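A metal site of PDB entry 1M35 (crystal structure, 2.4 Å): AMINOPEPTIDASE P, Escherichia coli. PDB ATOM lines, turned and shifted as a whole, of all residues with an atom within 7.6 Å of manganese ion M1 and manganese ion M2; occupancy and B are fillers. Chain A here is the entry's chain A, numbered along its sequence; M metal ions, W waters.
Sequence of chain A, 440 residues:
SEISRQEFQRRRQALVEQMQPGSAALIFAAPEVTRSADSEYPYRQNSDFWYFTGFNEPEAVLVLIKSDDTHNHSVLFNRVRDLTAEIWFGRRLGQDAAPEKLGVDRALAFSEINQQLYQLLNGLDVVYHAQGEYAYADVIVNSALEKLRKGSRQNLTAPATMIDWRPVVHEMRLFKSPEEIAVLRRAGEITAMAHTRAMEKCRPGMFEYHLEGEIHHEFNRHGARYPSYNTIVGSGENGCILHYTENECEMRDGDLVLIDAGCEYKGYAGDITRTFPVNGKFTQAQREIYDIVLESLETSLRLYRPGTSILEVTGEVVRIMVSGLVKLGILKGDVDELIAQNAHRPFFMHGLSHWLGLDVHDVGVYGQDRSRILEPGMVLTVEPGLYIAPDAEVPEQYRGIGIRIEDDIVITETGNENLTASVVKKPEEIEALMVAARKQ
OD2 of Asp 408 sits at hydrogen-bond distance from N of Asp 271, at 2.9 Å.
O of His 354 is in hydrogen-bond range of N of Thr 381.
The side-chain carboxylate (OE1) of Glu 383 lies within salt-bridge range of the guanidinium group (NE) of Arg 404 (3.9 Å).
The backbone NH (N) of Glu 383 lies within hydrogen-bond range of the backbone carbonyl oxygen (O) of Leu 352, at 2.8 Å.
The backbone carbonyl oxygen (O) of Asp 260 is in hydrogen-bond range of the backbone NH (N) of Ile 232 (2.9 Å).
The side-chain hydroxyl of Thr 273 sits at hydrogen-bond distance from the guanidinium group of Arg 404 (3.3 Å).
N of Ala 261 sits close to OH of Tyr 229.
The side-chain hydroxyl of Tyr 229 lies within hydrogen-bond range of the backbone NH of Gly 262 (3.0 Å).
Manganese ion M1 is bound by the side-chain carboxylate (OD2) of Asp 271 (2.0 Å), water W2 (2.0 Å), a ring nitrogen (NE2) of His 354 (2.1 Å), the side-chain carboxylate (OE2) of Glu 406 (2.1 Å) and the side-chain carboxylate (OE2) of Glu 383 (2.3 Å).
Manganese ion M1 has five donor atoms within binding distance.
Manganese ion M2 is bound by OD1 of Asp 271 (2.0 Å), water W2 (2.1 Å), OE1 of Glu 406 (2.2 Å), OD2 of Asp 260 (2.3 Å), OD1 of Asp 260 (2.3 Å) and water W1 (2.4 Å).
Manganese ion M2 has six donor atoms within binding distance.
Tyr 229 touches manganese ion M2.
OG1 of Thr 273 touches manganese ion M2, at 3.6 Å.
OG1 of Thr 381 touches manganese ion M1, at 3.9 Å.
Of the 26 residues printed, 5 come within 4 Å of manganese ion M1.
The nearest printed residue that does not touch manganese ion M1 is His 361 (4.7 Å).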
ATOM      1  N   TYR A 229       5.649  15.872  -2.468  1.00  0.00           N
ATOM      2  CA  TYR A 229       5.225  17.248  -2.244  1.00  0.00           C
ATOM      3  C   TYR A 229       6.385  17.980  -1.594  1.00  0.00           C
ATOM      4  O   TYR A 229       7.332  17.351  -1.121  1.00  0.00           O
ATOM      5  CB  TYR A 229       3.993  17.334  -1.332  1.00  0.00           C
ATOM      6  CG  TYR A 229       4.142  16.622  -0.011  1.00  0.00           C
ATOM      7  CD1 TYR A 229       3.916  15.239   0.094  1.00  0.00           C
ATOM      8  CD2 TYR A 229       4.551  17.310   1.133  1.00  0.00           C
ATOM      9  CE1 TYR A 229       4.078  14.564   1.310  1.00  0.00           C
ATOM     10  CE2 TYR A 229       4.718  16.648   2.360  1.00  0.00           C
ATOM     11  CZ  TYR A 229       4.477  15.269   2.439  1.00  0.00           C
ATOM     12  OH  TYR A 229       4.643  14.611   3.634  1.00  0.00           O
ATOM     13  N   ILE A 232       8.339  20.125   4.377  1.00  0.00           N
ATOM     14  CA  ILE A 232       8.112  21.160   5.368  1.00  0.00           C
ATOM     15  C   ILE A 232       8.948  20.873   6.612  1.00  0.00           C
ATOM     16  O   ILE A 232       8.860  19.776   7.188  1.00  0.00           O
ATOM     17  CB  ILE A 232       6.641  21.218   5.783  1.00  0.00           C
ATOM     18  CG1 ILE A 232       5.789  21.661   4.599  1.00  0.00           C
ATOM     19  CG2 ILE A 232       6.457  22.141   6.975  1.00  0.00           C
ATOM     20  CD1 ILE A 232       4.296  21.602   4.890  1.00  0.00           C
ATOM     21  N   ILE A 259       8.111  18.314  11.036  1.00  0.00           N
ATOM     22  CA  ILE A 259       8.535  17.867   9.724  1.00  0.00           C
ATOM     23  C   ILE A 259       7.461  17.078   9.004  1.00  0.00           C
ATOM     24  O   ILE A 259       7.044  16.018   9.468  1.00  0.00           O
ATOM     25  CB  ILE A 259       9.791  16.975   9.793  1.00  0.00           C
ATOM     26  CG1 ILE A 259      10.953  17.744  10.437  1.00  0.00           C
ATOM     27  CG2 ILE A 259      10.181  16.505   8.403  1.00  0.00           C
ATOM     28  CD1 ILE A 259      12.235  16.928  10.516  1.00  0.00           C
ATOM     29  N   ASP A 260       7.004  17.615   7.870  1.00  0.00           N
ATOM     30  CA  ASP A 260       6.009  16.945   7.057  1.00  0.00           C
ATOM     31  C   ASP A 260       6.706  16.677   5.728  1.00  0.00           C
ATOM     32  O   ASP A 260       7.029  17.611   4.993  1.00  0.00           O
ATOM     33  CB  ASP A 260       4.787  17.844   6.843  1.00  0.00           C
ATOM     34  CG  ASP A 260       3.600  17.079   6.271  1.00  0.00           C
ATOM     35  OD1 ASP A 260       3.813  16.013   5.664  1.00  0.00           O
ATOM     36  OD2 ASP A 260       2.458  17.554   6.414  1.00  0.00           O
ATOM     37  N   ALA A 261       6.968  15.410   5.440  1.00  0.00           N
ATOM     38  CA  ALA A 261       7.644  15.041   4.210  1.00  0.00           C
ATOM     39  C   ALA A 261       7.233  13.639   3.789  1.00  0.00           C
ATOM     40  O   ALA A 261       6.949  12.787   4.632  1.00  0.00           O
ATOM     41  CB  ALA A 261       9.144  15.110   4.404  1.00  0.00           C
ATOM     42  N   GLY A 262       7.193  13.422   2.475  1.00  0.00           N
ATOM     43  CA  GLY A 262       6.811  12.137   1.942  1.00  0.00           C
ATOM     44  C   GLY A 262       7.494  11.920   0.607  1.00  0.00           C
ATOM     45  O   GLY A 262       7.694  12.852  -0.176  1.00  0.00           O
ATOM     46  N   GLY A 270       3.959   9.012  -0.071  1.00  0.00           N
ATOM     47  CA  GLY A 270       4.021   8.718   1.338  1.00  0.00           C
ATOM     48  C   GLY A 270       3.707  10.103   1.895  1.00  0.00           C
ATOM     49  O   GLY A 270       3.942  11.099   1.196  1.00  0.00           O
ATOM     50  N   ASP A 271       3.171  10.191   3.102  1.00  0.00           N
ATOM     51  CA  ASP A 271       2.846  11.495   3.675  1.00  0.00           C
ATOM     52  C   ASP A 271       2.900  11.365   5.186  1.00  0.00           C
ATOM     53  O   ASP A 271       1.929  10.956   5.820  1.00  0.00           O
ATOM     54  CB  ASP A 271       1.447  11.965   3.218  1.00  0.00           C
ATOM     55  CG  ASP A 271       1.044  13.337   3.788  1.00  0.00           C
ATOM     56  OD1 ASP A 271       1.867  14.019   4.421  1.00  0.00           O
ATOM     57  OD2 ASP A 271      -0.129  13.745   3.588  1.00  0.00           O
ATOM     58  N   ILE A 272       4.060  11.701   5.756  1.00  0.00           N
ATOM     59  CA  ILE A 272       4.258  11.599   7.192  1.00  0.00           C
ATOM     60  C   ILE A 272       4.608  12.915   7.864  1.00  0.00           C
ATOM     61  O   ILE A 272       5.331  13.729   7.301  1.00  0.00           O
ATOM     62  CB  ILE A 272       5.409  10.611   7.534  1.00  0.00           C
ATOM     63  CG1 ILE A 272       5.021   9.179   7.164  1.00  0.00           C
ATOM     64  CG2 ILE A 272       5.774  10.709   9.028  1.00  0.00           C
ATOM     65  CD1 ILE A 272       6.104   8.133   7.523  1.00  0.00           C
ATOM     66  N   THR A 273       4.096  13.117   9.066  1.00  0.00           N
ATOM     67  CA  THR A 273       4.437  14.305   9.826  1.00  0.00           C
ATOM     68  C   THR A 273       4.847  13.837  11.218  1.00  0.00           C
ATOM     69  O   THR A 273       4.188  12.992  11.821  1.00  0.00           O
ATOM     70  CB  THR A 273       3.276  15.304  10.012  1.00  0.00           C
ATOM     71  OG1 THR A 273       2.782  15.748   8.744  1.00  0.00           O
ATOM     72  CG2 THR A 273       3.768  16.513  10.784  1.00  0.00           C
ATOM     73  N   GLY A 351      -8.344  19.651   8.032  1.00  0.00           N
ATOM     74  CA  GLY A 351      -9.001  18.355   8.126  1.00  0.00           C
ATOM     75  C   GLY A 351      -8.163  17.302   8.817  1.00  0.00           C
ATOM     76  O   GLY A 351      -6.933  17.425   8.905  1.00  0.00           O
ATOM     77  N   LEU A 352      -8.819  16.249   9.289  1.00  0.00           N
ATOM     78  CA  LEU A 352      -8.131  15.174   9.968  1.00  0.00           C
ATOM     79  C   LEU A 352      -7.523  14.199   8.971  1.00  0.00           C
ATOM     80  O   LEU A 352      -6.449  13.644   9.212  1.00  0.00           O
ATOM     81  CB  LEU A 352      -9.097  14.421  10.874  1.00  0.00           C
ATOM     82  CG  LEU A 352      -8.506  13.242  11.647  1.00  0.00           C
ATOM     83  CD1 LEU A 352      -7.477  13.737  12.654  1.00  0.00           C
ATOM     84  CD2 LEU A 352      -9.642  12.492  12.348  1.00  0.00           C
ATOM     85  N   SER A 353      -8.205  13.990   7.843  1.00  0.00           N
ATOM     86  CA  SER A 353      -7.742  13.033   6.849  1.00  0.00           C
ATOM     87  C   SER A 353      -8.023  13.398   5.401  1.00  0.00           C
ATOM     88  O   SER A 353      -8.984  14.108   5.101  1.00  0.00           O
ATOM     89  CB  SER A 353      -8.401  11.664   7.094  1.00  0.00           C
ATOM     90  OG  SER A 353      -8.228  11.222   8.426  1.00  0.00           O
ATOM     91  N   HIS A 354      -7.175  12.900   4.504  1.00  0.00           N
ATOM     92  CA  HIS A 354      -7.357  13.086   3.074  1.00  0.00           C
ATOM     93  C   HIS A 354      -6.937  11.797   2.381  1.00  0.00           C
ATOM     94  O   HIS A 354      -6.095  11.062   2.918  1.00  0.00           O
ATOM     95  CB  HIS A 354      -6.555  14.298   2.560  1.00  0.00           C
ATOM     96  CG  HIS A 354      -5.071  14.161   2.703  1.00  0.00           C
ATOM     97  ND1 HIS A 354      -4.289  13.295   1.975  1.00  0.00           N
ATOM     98  CD2 HIS A 354      -4.208  14.844   3.499  1.00  0.00           C
ATOM     99  CE1 HIS A 354      -3.011  13.465   2.345  1.00  0.00           C
ATOM    100  NE2 HIS A 354      -2.905  14.391   3.271  1.00  0.00           N
ATOM    101  N   TRP A 355      -7.541  11.488   1.239  1.00  0.00           N
ATOM    102  CA  TRP A 355      -7.193  10.274   0.496  1.00  0.00           C
ATOM    103  C   TRP A 355      -5.715  10.337   0.133  1.00  0.00           C
ATOM    104  O   TRP A 355      -5.134  11.418   0.056  1.00  0.00           O
ATOM    105  CB  TRP A 355      -8.016  10.153  -0.792  1.00  0.00           C
ATOM    106  CG  TRP A 355      -9.521  10.238  -0.643  1.00  0.00           C
ATOM    107  CD1 TRP A 355     -10.358  11.051  -1.354  1.00  0.00           C
ATOM    108  CD2 TRP A 355     -10.357   9.472   0.235  1.00  0.00           C
ATOM    109  NE1 TRP A 355     -11.665  10.844  -0.973  1.00  0.00           N
ATOM    110  CE2 TRP A 355     -11.695   9.877  -0.001  1.00  0.00           C
ATOM    111  CE3 TRP A 355     -10.114   8.482   1.200  1.00  0.00           C
ATOM    112  CZ2 TRP A 355     -12.779   9.326   0.694  1.00  0.00           C
ATOM    113  CZ3 TRP A 355     -11.192   7.939   1.893  1.00  0.00           C
ATOM    114  CH2 TRP A 355     -12.509   8.360   1.637  1.00  0.00           C
ATOM    115  N   LEU A 356      -5.102   9.182  -0.123  1.00  0.00           N
ATOM    116  CA  LEU A 356      -3.700   9.119  -0.488  1.00  0.00           C
ATOM    117  C   LEU A 356      -3.530   8.125  -1.638  1.00  0.00           C
ATOM    118  O   LEU A 356      -4.191   7.084  -1.659  1.00  0.00           O
ATOM    119  CB  LEU A 356      -2.868   8.673   0.719  1.00  0.00           C
ATOM    120  CG  LEU A 356      -1.347   8.685   0.577  1.00  0.00           C
ATOM    121  CD1 LEU A 356      -0.858  10.134   0.500  1.00  0.00           C
ATOM    122  CD2 LEU A 356      -0.706   7.977   1.764  1.00  0.00           C
ATOM    123  N   VAL A 360      -0.604  13.074  -3.392  1.00  0.00           N
ATOM    124  CA  VAL A 360      -0.637  13.150  -1.946  1.00  0.00           C
ATOM    125  C   VAL A 360      -2.057  13.459  -1.458  1.00  0.00           C
ATOM    126  O   VAL A 360      -2.511  12.870  -0.473  1.00  0.00           O
ATOM    127  CB  VAL A 360       0.408  14.159  -1.391  1.00  0.00           C
ATOM    128  CG1 VAL A 360       0.107  15.570  -1.880  1.00  0.00           C
ATOM    129  CG2 VAL A 360       0.412  14.106   0.139  1.00  0.00           C
ATOM    130  N   HIS A 361      -2.747  14.375  -2.128  1.00  0.00           N
ATOM    131  CA  HIS A 361      -4.141  14.704  -1.813  1.00  0.00           C
ATOM    132  C   HIS A 361      -4.878  13.995  -2.939  1.00  0.00           C
ATOM    133  O   HIS A 361      -5.265  14.613  -3.924  1.00  0.00           O
ATOM    134  CB  HIS A 361      -4.382  16.206  -1.890  1.00  0.00           C
ATOM    135  CG  HIS A 361      -3.735  16.963  -0.775  1.00  0.00           C
ATOM    136  ND1 HIS A 361      -3.573  18.330  -0.765  1.00  0.00           N
ATOM    137  CD2 HIS A 361      -3.201  16.519   0.390  1.00  0.00           C
ATOM    138  CE1 HIS A 361      -2.958  18.659   0.386  1.00  0.00           C
ATOM    139  NE2 HIS A 361      -2.705  17.585   1.111  1.00  0.00           N
ATOM    140  N   LEU A 380      -5.933   6.578   3.351  1.00  0.00           N
ATOM    141  CA  LEU A 380      -6.034   7.949   3.810  1.00  0.00           C
ATOM    142  C   LEU A 380      -5.017   8.260   4.895  1.00  0.00           C
ATOM    143  O   LEU A 380      -4.409   7.361   5.476  1.00  0.00           O
ATOM    144  CB  LEU A 380      -7.436   8.215   4.385  1.00  0.00           C
ATOM    145  CG  LEU A 380      -7.856   7.297   5.548  1.00  0.00           C
ATOM    146  CD1 LEU A 380      -8.896   7.984   6.424  1.00  0.00           C
ATOM    147  CD2 LEU A 380      -8.388   5.975   5.000  1.00  0.00           C
ATOM    148  N   THR A 381      -4.848   9.542   5.176  1.00  0.00           N
ATOM    149  CA  THR A 381      -3.923   9.973   6.207  1.00  0.00           C
ATOM    150  C   THR A 381      -4.716  10.276   7.468  1.00  0.00           C
ATOM    151  O   THR A 381      -5.946  10.380   7.443  1.00  0.00           O
ATOM    152  CB  THR A 381      -3.181  11.276   5.812  1.00  0.00           C
ATOM    153  OG1 THR A 381      -4.131  12.327   5.623  1.00  0.00           O
ATOM    154  CG2 THR A 381      -2.387  11.071   4.520  1.00  0.00           C
ATOM    155  N   VAL A 382      -4.009  10.378   8.586  1.00  0.00           N
ATOM    156  CA  VAL A 382      -4.616  10.715   9.864  1.00  0.00           C
ATOM    157  C   VAL A 382      -3.638  11.736  10.401  1.00  0.00           C
ATOM    158  O   VAL A 382      -2.532  11.375  10.820  1.00  0.00           O
ATOM    159  CB  VAL A 382      -4.679   9.496  10.810  1.00  0.00           C
ATOM    160  CG1 VAL A 382      -5.528   9.831  12.016  1.00  0.00           C
ATOM    161  CG2 VAL A 382      -5.237   8.285  10.064  1.00  0.00           C
ATOM    162  N   GLU A 383      -4.032  12.998  10.390  1.00  0.00           N
ATOM    163  CA  GLU A 383      -3.101  14.029  10.827  1.00  0.00           C
ATOM    164  C   GLU A 383      -3.625  15.108  11.737  1.00  0.00           C
ATOM    165  O   GLU A 383      -3.717  16.273  11.356  1.00  0.00           O
ATOM    166  CB  GLU A 383      -2.449  14.665   9.589  1.00  0.00           C
ATOM    167  CG  GLU A 383      -3.422  15.124   8.509  1.00  0.00           C
ATOM    168  CD  GLU A 383      -2.729  15.526   7.207  1.00  0.00           C
ATOM    169  OE1 GLU A 383      -1.867  16.435   7.244  1.00  0.00           O
ATOM    170  OE2 GLU A 383      -3.026  14.933   6.157  1.00  0.00           O
ATOM    171  N   ARG A 404       2.000  18.539  14.897  1.00  0.00           N
ATOM    172  CA  ARG A 404       1.185  17.688  14.056  1.00  0.00           C
ATOM    173  C   ARG A 404       1.862  16.330  13.984  1.00  0.00           C
ATOM    174  O   ARG A 404       3.092  16.249  13.908  1.00  0.00           O
ATOM    175  CB  ARG A 404       1.027  18.271  12.647  1.00  0.00           C
ATOM    176  CG  ARG A 404       0.252  17.346  11.724  1.00  0.00           C
ATOM    177  CD  ARG A 404      -0.259  18.007  10.445  1.00  0.00           C
ATOM    178  NE  ARG A 404       0.783  18.302   9.474  1.00  0.00           N
ATOM    179  CZ  ARG A 404       1.280  19.521   9.259  1.00  0.00           C
ATOM    180  NH1 ARG A 404       0.819  20.555   9.941  1.00  0.00           N
ATOM    181  NH2 ARG A 404       2.218  19.690   8.336  1.00  0.00           N
ATOM    182  N   GLU A 406       1.324  12.710  11.831  1.00  0.00           N
ATOM    183  CA  GLU A 406       0.554  12.125  10.745  1.00  0.00           C
ATOM    184  C   GLU A 406       1.031  10.754  10.250  1.00  0.00           C
ATOM    185  O   GLU A 406       2.209  10.558  10.009  1.00  0.00           O
ATOM    186  CB  GLU A 406       0.526  13.119   9.567  1.00  0.00           C
ATOM    187  CG  GLU A 406       0.171  12.544   8.193  1.00  0.00           C
ATOM    188  CD  GLU A 406       0.140  13.619   7.089  1.00  0.00           C
ATOM    189  OE1 GLU A 406       1.028  14.506   7.084  1.00  0.00           O
ATOM    190  OE2 GLU A 406      -0.759  13.558   6.213  1.00  0.00           O
ATOM    191  N   ASP A 407       0.096   9.825  10.123  1.00  0.00           N
ATOM    192  CA  ASP A 407       0.383   8.482   9.623  1.00  0.00           C
ATOM    193  C   ASP A 407      -0.503   8.208   8.413  1.00  0.00           C
ATOM    194  O   ASP A 407      -1.503   8.898   8.201  1.00  0.00           O
ATOM    195  CB  ASP A 407       0.093   7.403  10.685  1.00  0.00           C
ATOM    196  CG  ASP A 407       1.223   7.230  11.681  1.00  0.00           C
ATOM    197  OD1 ASP A 407       2.405   7.385  11.302  1.00  0.00           O
ATOM    198  OD2 ASP A 407       0.925   6.907  12.857  1.00  0.00           O
ATOM    199  N   ASP A 408      -0.129   7.192   7.632  1.00  0.00           N
ATOM    200  CA  ASP A 408      -0.895   6.822   6.454  1.00  0.00           C
ATOM    201  C   ASP A 408      -1.459   5.427   6.710  1.00  0.00           C
ATOM    202  O   ASP A 408      -0.710   4.523   7.106  1.00  0.00           O
ATOM    203  CB  ASP A 408      -0.013   6.796   5.191  1.00  0.00           C
ATOM    204  CG  ASP A 408       0.797   8.069   5.020  1.00  0.00           C
ATOM    205  OD1 ASP A 408       0.324   9.157   5.451  1.00  0.00           O
ATOM    206  OD2 ASP A 408       1.901   8.007   4.438  1.00  0.00           O
HETATM  207 MN    MN M   1      -1.365  14.826   4.642  1.00  0.00          MN
HETATM  208 MN    MN M   2       1.556  15.748   5.384  1.00  0.00          MN
HETATM  209  O   HOH W   1       1.667  16.888   3.239  1.00  0.00           O
HETATM  210  O   HOH W   2      -0.386  16.421   5.220  1.00  0.00           O
HETATM  211  O   HOH W   3      -0.933  17.917   3.366  1.00  0.00           O
